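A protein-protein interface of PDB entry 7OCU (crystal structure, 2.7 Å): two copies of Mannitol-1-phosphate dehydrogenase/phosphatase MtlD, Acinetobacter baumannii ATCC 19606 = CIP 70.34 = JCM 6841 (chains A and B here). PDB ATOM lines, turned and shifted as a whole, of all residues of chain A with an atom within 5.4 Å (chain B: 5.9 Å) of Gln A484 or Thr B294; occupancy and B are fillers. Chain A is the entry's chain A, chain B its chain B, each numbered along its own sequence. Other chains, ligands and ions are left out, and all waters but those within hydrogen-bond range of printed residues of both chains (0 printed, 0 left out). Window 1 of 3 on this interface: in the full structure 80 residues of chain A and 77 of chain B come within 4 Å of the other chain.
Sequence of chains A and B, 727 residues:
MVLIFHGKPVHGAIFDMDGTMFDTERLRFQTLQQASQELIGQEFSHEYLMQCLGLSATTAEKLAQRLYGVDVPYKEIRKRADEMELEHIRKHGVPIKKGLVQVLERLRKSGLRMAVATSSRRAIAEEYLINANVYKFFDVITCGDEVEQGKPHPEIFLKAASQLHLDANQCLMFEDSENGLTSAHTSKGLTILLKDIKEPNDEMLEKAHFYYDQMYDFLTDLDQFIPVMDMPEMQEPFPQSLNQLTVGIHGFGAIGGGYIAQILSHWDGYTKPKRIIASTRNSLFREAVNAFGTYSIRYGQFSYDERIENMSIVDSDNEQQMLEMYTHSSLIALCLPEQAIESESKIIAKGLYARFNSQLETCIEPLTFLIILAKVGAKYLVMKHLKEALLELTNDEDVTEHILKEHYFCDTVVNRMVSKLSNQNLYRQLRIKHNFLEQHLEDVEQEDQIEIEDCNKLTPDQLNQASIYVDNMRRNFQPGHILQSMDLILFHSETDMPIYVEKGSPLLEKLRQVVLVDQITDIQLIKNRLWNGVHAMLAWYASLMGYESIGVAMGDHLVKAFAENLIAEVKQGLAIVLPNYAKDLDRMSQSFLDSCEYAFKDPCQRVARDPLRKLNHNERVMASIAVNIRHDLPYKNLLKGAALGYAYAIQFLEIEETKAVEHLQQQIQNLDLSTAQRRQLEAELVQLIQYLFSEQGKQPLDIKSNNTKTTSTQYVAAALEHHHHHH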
ATOM      1  N   ARG A 307      18.748 -13.655 -22.210  1.00  0.00           N
ATOM      2  CA  ARG A 307      19.719 -13.524 -21.088  1.00  0.00           C
ATOM      3  C   ARG A 307      20.792 -12.493 -21.462  1.00  0.00           C
ATOM      4  O   ARG A 307      21.504 -12.716 -22.457  1.00  0.00           O
ATOM      5  CB  ARG A 307      20.327 -14.891 -20.755  1.00  0.00           C
ATOM      6  CG  ARG A 307      21.335 -14.872 -19.613  1.00  0.00           C
ATOM      7  CD  ARG A 307      21.049 -15.914 -18.546  1.00  0.00           C
ATOM      8  NE  ARG A 307      20.957 -17.272 -19.069  1.00  0.00           N
ATOM      9  CZ  ARG A 307      20.528 -18.329 -18.381  1.00  0.00           C
ATOM     10  NH1 ARG A 307      20.483 -19.518 -18.961  1.00  0.00           N
ATOM     11  NH2 ARG A 307      20.143 -18.202 -17.120  1.00  0.00           N
ATOM     12  N   GLY A 480      26.399 -23.492  -8.896  1.00  0.00           N
ATOM     13  CA  GLY A 480      25.943 -22.631 -10.007  1.00  0.00           C
ATOM     14  C   GLY A 480      25.588 -23.411 -11.267  1.00  0.00           C
ATOM     15  O   GLY A 480      25.460 -22.768 -12.327  1.00  0.00           O
ATOM     16  N   HIS A 481      25.432 -24.738 -11.168  1.00  0.00           N
ATOM     17  CA  HIS A 481      24.983 -25.631 -12.274  1.00  0.00           C
ATOM     18  C   HIS A 481      23.524 -25.329 -12.633  1.00  0.00           C
ATOM     19  O   HIS A 481      23.172 -25.453 -13.824  1.00  0.00           O
ATOM     20  CB  HIS A 481      25.156 -27.110 -11.894  1.00  0.00           C
ATOM     21  CG  HIS A 481      26.536 -27.631 -12.105  1.00  0.00           C
ATOM     22  ND1 HIS A 481      27.646 -26.812 -12.076  1.00  0.00           N
ATOM     23  CD2 HIS A 481      26.992 -28.883 -12.336  1.00  0.00           C
ATOM     24  CE1 HIS A 481      28.726 -27.532 -12.288  1.00  0.00           C
ATOM     25  NE2 HIS A 481      28.353 -28.807 -12.450  1.00  0.00           N
ATOM     26  N   ILE A 482      22.717 -24.953 -11.635  1.00  0.00           N
ATOM     27  CA  ILE A 482      21.249 -24.694 -11.759  1.00  0.00           C
ATOM     28  C   ILE A 482      21.005 -23.505 -12.703  1.00  0.00           C
ATOM     29  O   ILE A 482      19.908 -23.450 -13.294  1.00  0.00           O
ATOM     30  CB  ILE A 482      20.616 -24.483 -10.366  1.00  0.00           C
ATOM     31  CG1 ILE A 482      19.093 -24.647 -10.389  1.00  0.00           C
ATOM     32  CG2 ILE A 482      21.028 -23.146  -9.766  1.00  0.00           C
ATOM     33  CD1 ILE A 482      18.628 -26.078 -10.528  1.00  0.00           C
ATOM     34  N   LEU A 483      21.985 -22.605 -12.854  1.00  0.00           N
ATOM     35  CA  LEU A 483      21.884 -21.377 -13.695  1.00  0.00           C
ATOM     36  C   LEU A 483      21.859 -21.729 -15.191  1.00  0.00           C
ATOM     37  O   LEU A 483      21.562 -20.819 -15.991  1.00  0.00           O
ATOM     38  CB  LEU A 483      23.054 -20.439 -13.377  1.00  0.00           C
ATOM     39  CG  LEU A 483      23.089 -19.864 -11.961  1.00  0.00           C
ATOM     40  CD1 LEU A 483      24.179 -18.809 -11.839  1.00  0.00           C
ATOM     41  CD2 LEU A 483      21.738 -19.280 -11.565  1.00  0.00           C
ATOM     42  N   GLN A 484      22.172 -22.980 -15.559  1.00  0.00           N
ATOM     43  CA  GLN A 484      22.033 -23.510 -16.947  1.00  0.00           C
ATOM     44  C   GLN A 484      20.618 -23.222 -17.464  1.00  0.00           C
ATOM     45  O   GLN A 484      20.497 -22.696 -18.590  1.00  0.00           O
ATOM     46  CB  GLN A 484      22.307 -25.016 -16.993  1.00  0.00           C
ATOM     47  CG  GLN A 484      23.787 -25.376 -16.999  1.00  0.00           C
ATOM     48  CD  GLN A 484      24.017 -26.869 -16.992  1.00  0.00           C
ATOM     49  OE1 GLN A 484      23.215 -27.648 -17.506  1.00  0.00           O
ATOM     50  NE2 GLN A 484      25.129 -27.283 -16.406  1.00  0.00           N
ATOM     51  N   SER A 485      19.600 -23.563 -16.664  1.00  0.00           N
ATOM     52  CA  SER A 485      18.155 -23.384 -16.970  1.00  0.00           C
ATOM     53  C   SER A 485      17.460 -22.687 -15.791  1.00  0.00           C
ATOM     54  O   SER A 485      16.568 -23.305 -15.174  1.00  0.00           O
ATOM     55  CB  SER A 485      17.514 -24.710 -17.298  1.00  0.00           C
ATOM     56  OG  SER A 485      16.133 -24.551 -17.593  1.00  0.00           O
ATOM     57  N   MET A 486      17.867 -21.448 -15.496  1.00  0.00           N
ATOM     58  CA  MET A 486      17.300 -20.600 -14.411  1.00  0.00           C
ATOM     59  C   MET A 486      17.625 -19.130 -14.698  1.00  0.00           C
ATOM     60  O   MET A 486      18.797 -18.740 -14.526  1.00  0.00           O
ATOM     61  CB  MET A 486      17.873 -20.999 -13.047  1.00  0.00           C
ATOM     62  CG  MET A 486      17.343 -20.163 -11.894  1.00  0.00           C
ATOM     63  SD  MET A 486      17.664 -20.917 -10.280  1.00  0.00           S
ATOM     64  CE  MET A 486      16.539 -22.311 -10.344  1.00  0.00           C
ATOM     65  N   ALA B 288      35.391 -34.097 -15.385  1.00  0.00           N
ATOM     66  CA  ALA B 288      35.543 -32.724 -15.924  1.00  0.00           C
ATOM     67  C   ALA B 288      34.173 -32.153 -16.312  1.00  0.00           C
ATOM     68  O   ALA B 288      33.867 -31.021 -15.890  1.00  0.00           O
ATOM     69  CB  ALA B 288      36.487 -32.727 -17.102  1.00  0.00           C
ATOM     70  N   VAL B 289      33.386 -32.908 -17.085  1.00  0.00           N
ATOM     71  CA  VAL B 289      32.045 -32.489 -17.597  1.00  0.00           C
ATOM     72  C   VAL B 289      31.099 -32.283 -16.408  1.00  0.00           C
ATOM     73  O   VAL B 289      30.364 -31.276 -16.413  1.00  0.00           O
ATOM     74  CB  VAL B 289      31.473 -33.507 -18.605  1.00  0.00           C
ATOM     75  CG1 VAL B 289      30.017 -33.219 -18.944  1.00  0.00           C
ATOM     76  CG2 VAL B 289      32.307 -33.573 -19.876  1.00  0.00           C
ATOM     77  N   PHE B 292      32.089 -29.084 -14.417  1.00  0.00           N
ATOM     78  CA  PHE B 292      31.688 -27.857 -15.160  1.00  0.00           C
ATOM     79  C   PHE B 292      30.161 -27.789 -15.281  1.00  0.00           C
ATOM     80  O   PHE B 292      29.605 -26.676 -15.180  1.00  0.00           O
ATOM     81  CB  PHE B 292      32.338 -27.814 -16.547  1.00  0.00           C
ATOM     82  CG  PHE B 292      33.640 -27.059 -16.611  1.00  0.00           C
ATOM     83  CD1 PHE B 292      34.829 -27.657 -16.219  1.00  0.00           C
ATOM     84  CD2 PHE B 292      33.680 -25.749 -17.066  1.00  0.00           C
ATOM     85  CE1 PHE B 292      36.026 -26.959 -16.279  1.00  0.00           C
ATOM     86  CE2 PHE B 292      34.878 -25.053 -17.125  1.00  0.00           C
ATOM     87  CZ  PHE B 292      36.049 -25.659 -16.731  1.00  0.00           C
ATOM     88  N   GLY B 293      29.516 -28.939 -15.506  1.00  0.00           N
ATOM     89  CA  GLY B 293      28.058 -29.063 -15.710  1.00  0.00           C
ATOM     90  C   GLY B 293      27.706 -29.114 -17.186  1.00  0.00           C
ATOM     91  O   GLY B 293      26.737 -29.816 -17.542  1.00  0.00           O
ATOM     92  N   THR B 294      28.462 -28.388 -18.015  1.00  0.00           N
ATOM     93  CA  THR B 294      28.322 -28.337 -19.493  1.00  0.00           C
ATOM     94  C   THR B 294      29.674 -28.644 -20.145  1.00  0.00           C
ATOM     95  O   THR B 294      30.694 -28.649 -19.429  1.00  0.00           O
ATOM     96  CB  THR B 294      27.805 -26.968 -19.950  1.00  0.00           C
ATOM     97  OG1 THR B 294      28.844 -26.010 -19.742  1.00  0.00           O
ATOM     98  CG2 THR B 294      26.556 -26.532 -19.215  1.00  0.00           C
ATOM     99  N   TYR B 295      29.661 -28.898 -21.455  1.00  0.00           N
ATOM    100  CA  TYR B 295      30.854 -28.975 -22.336  1.00  0.00           C
ATOM    101  C   TYR B 295      30.473 -28.397 -23.703  1.00  0.00           C
ATOM    102  O   TYR B 295      29.285 -28.478 -24.076  1.00  0.00           O
ATOM    103  CB  TYR B 295      31.363 -30.415 -22.445  1.00  0.00           C
ATOM    104  CG  TYR B 295      30.549 -31.298 -23.355  1.00  0.00           C
ATOM    105  CD1 TYR B 295      30.819 -31.366 -24.713  1.00  0.00           C
ATOM    106  CD2 TYR B 295      29.498 -32.056 -22.864  1.00  0.00           C
ATOM    107  CE1 TYR B 295      30.070 -32.166 -25.559  1.00  0.00           C
ATOM    108  CE2 TYR B 295      28.742 -32.863 -23.698  1.00  0.00           C
ATOM    109  CZ  TYR B 295      29.027 -32.919 -25.050  1.00  0.00           C
ATOM    110  OH  TYR B 295      28.282 -33.714 -25.868  1.00  0.00           O
ATOM    111  N   SER B 296      31.448 -27.837 -24.423  1.00  0.00           N
ATOM    112  CA  SER B 296      31.252 -27.169 -25.735  1.00  0.00           C
ATOM    113  C   SER B 296      31.896 -27.994 -26.855  1.00  0.00           C
ATOM    114  O   SER B 296      32.965 -28.591 -26.614  1.00  0.00           O
ATOM    115  CB  SER B 296      31.790 -25.764 -25.706  1.00  0.00           C
ATOM    116  OG  SER B 296      30.997 -24.937 -24.865  1.00  0.00           O
ATOM    117  N   ARG B 307      27.822 -24.865 -26.709  1.00  0.00           N
ATOM    118  CA  ARG B 307      27.661 -25.384 -25.324  1.00  0.00           C
ATOM    119  C   ARG B 307      26.526 -26.415 -25.299  1.00  0.00           C
ATOM    120  O   ARG B 307      25.402 -26.065 -25.711  1.00  0.00           O
ATOM    121  CB  ARG B 307      27.386 -24.230 -24.353  1.00  0.00           C
ATOM    122  CG  ARG B 307      27.099 -24.667 -22.923  1.00  0.00           C
ATOM    123  CD  ARG B 307      26.745 -23.513 -22.002  1.00  0.00           C
ATOM    124  NE  ARG B 307      27.914 -22.921 -21.360  1.00  0.00           N
ATOM    125  CZ  ARG B 307      28.611 -21.879 -21.813  1.00  0.00           C
ATOM    126  NH1 ARG B 307      29.652 -21.440 -21.126  1.00  0.00           N
ATOM    127  NH2 ARG B 307      28.276 -21.274 -22.942  1.00  0.00           N
ATOM    128  N   ILE B 308      26.820 -27.633 -24.832  1.00  0.00           N
ATOM    129  CA  ILE B 308      25.831 -28.727 -24.590  1.00  0.00           C
ATOM    130  C   ILE B 308      25.543 -28.782 -23.084  1.00  0.00           C
ATOM    131  O   ILE B 308      26.470 -29.120 -22.321  1.00  0.00           O
ATOM    132  CB  ILE B 308      26.350 -30.080 -25.124  1.00  0.00           C
ATOM    133  CG1 ILE B 308      26.877 -29.975 -26.560  1.00  0.00           C
ATOM    134  CG2 ILE B 308      25.282 -31.156 -24.996  1.00  0.00           C
ATOM    135  CD1 ILE B 308      25.849 -29.517 -27.573  1.00  0.00           C
ATOM    136  N   GLU B 309      24.307 -28.465 -22.684  1.00  0.00           N
ATOM    137  CA  GLU B 309      23.871 -28.393 -21.262  1.00  0.00           C
ATOM    138  C   GLU B 309      22.893 -29.538 -20.969  1.00  0.00           C
ATOM    139  O   GLU B 309      22.458 -30.204 -21.930  1.00  0.00           O
ATOM    140  CB  GLU B 309      23.274 -27.015 -20.958  1.00  0.00           C
ATOM    141  CG  GLU B 309      21.991 -26.703 -21.714  1.00  0.00           C
ATOM    142  CD  GLU B 309      21.565 -25.244 -21.683  1.00  0.00           C
ATOM    143  OE1 GLU B 309      22.438 -24.370 -21.485  1.00  0.00           O
ATOM    144  OE2 GLU B 309      20.356 -24.982 -21.858  1.00  0.00           O
ATOM    145  N   ASN B 310      22.585 -29.756 -19.686  1.00  0.00           N
ATOM    146  CA  ASN B 310      21.730 -30.865 -19.176  1.00  0.00           C
ATOM    147  C   ASN B 310      22.437 -32.205 -19.419  1.00  0.00           C
ATOM    148  O   ASN B 310      21.749 -33.182 -19.780  1.00  0.00           O
ATOM    149  CB  ASN B 310      20.335 -30.851 -19.810  1.00  0.00           C
ATOM    150  CG  ASN B 310      19.651 -29.504 -19.713  1.00  0.00           C
ATOM    151  OD1 ASN B 310      19.784 -28.805 -18.711  1.00  0.00           O
ATOM    152  ND2 ASN B 310      18.914 -29.137 -20.748  1.00  0.00           N
ATOM    153  N   MET B 311      23.758 -32.247 -19.214  1.00  0.00           N
ATOM    154  CA  MET B 311      24.619 -33.435 -19.463  1.00  0.00           C
ATOM    155  C   MET B 311      24.979 -34.098 -18.129  1.00  0.00           C
ATOM    156  O   MET B 311      25.349 -33.370 -17.185  1.00  0.00           O
ATOM    157  CB  MET B 311      25.911 -33.037 -20.184  1.00  0.00           C
ATOM    158  CG  MET B 311      25.716 -32.686 -21.650  1.00  0.00           C
ATOM    159  SD  MET B 311      25.217 -34.087 -22.695  1.00  0.00           S
ATOM    160  CE  MET B 311      26.356 -35.361 -22.154  1.00  0.00           C
ATOM    161  N   LEU B 488      34.224 -25.416 -21.538  1.00  0.00           N
ATOM    162  CA  LEU B 488      35.070 -26.639 -21.555  1.00  0.00           C
ATOM    163  C   LEU B 488      35.004 -27.261 -22.956  1.00  0.00           C
ATOM    164  O   LEU B 488      33.962 -27.858 -23.291  1.00  0.00           O
ATOM    165  CB  LEU B 488      34.574 -27.612 -20.480  1.00  0.00           C
ATOM    166  CG  LEU B 488      35.427 -28.862 -20.277  1.00  0.00           C
ATOM    167  CD1 LEU B 488      36.785 -28.507 -19.688  1.00  0.00           C
ATOM    168  CD2 LEU B 488      34.710 -29.867 -19.388  1.00  0.00           C
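The backbone NH (N) of Asn B310 lies within hydrogen-bond range of the side-chain amide oxygen (OE1) of Gln A484 (3.1 Å). The backbone NH (N) of Gly B293 lies within hydrogen-bond range of a ring nitrogen (NE2) of His A481, 3.3 Å away. The backbone carbonyl oxygen of Gly B293 is in hydrogen-bond range of the side-chain amide nitrogen of Gln A484, at 3.2 Å.
The guanidinium group (NH1) of Arg A307 lies within hydrogen-bond range of the backbone carbonyl oxygen (O) of Gln A484 (3.2 Å).
His A481 touches Phe B292 (CE1 to O, 3.1 Å). CG2 of Thr B294 touches NE2 of Gln A484, 3.2 Å away. CB of Glu B309 touches OE1 of Gln A484 (3.5 Å).
Gln A484 touches four residues of chain B. Of the printed residues of chain A, Glu B309 touches Gln A484. Printed residues of chain B within 4 Å of His A481: Phe B292 and Gly B293. Tyr B295 touches none of the printed residues of chain A.
Among the printed residues, no Asp or Glu carboxylate lies within 4 Å of a Lys or Arg side-chain nitrogen of the other chain.
Position printed for both chains: 307.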
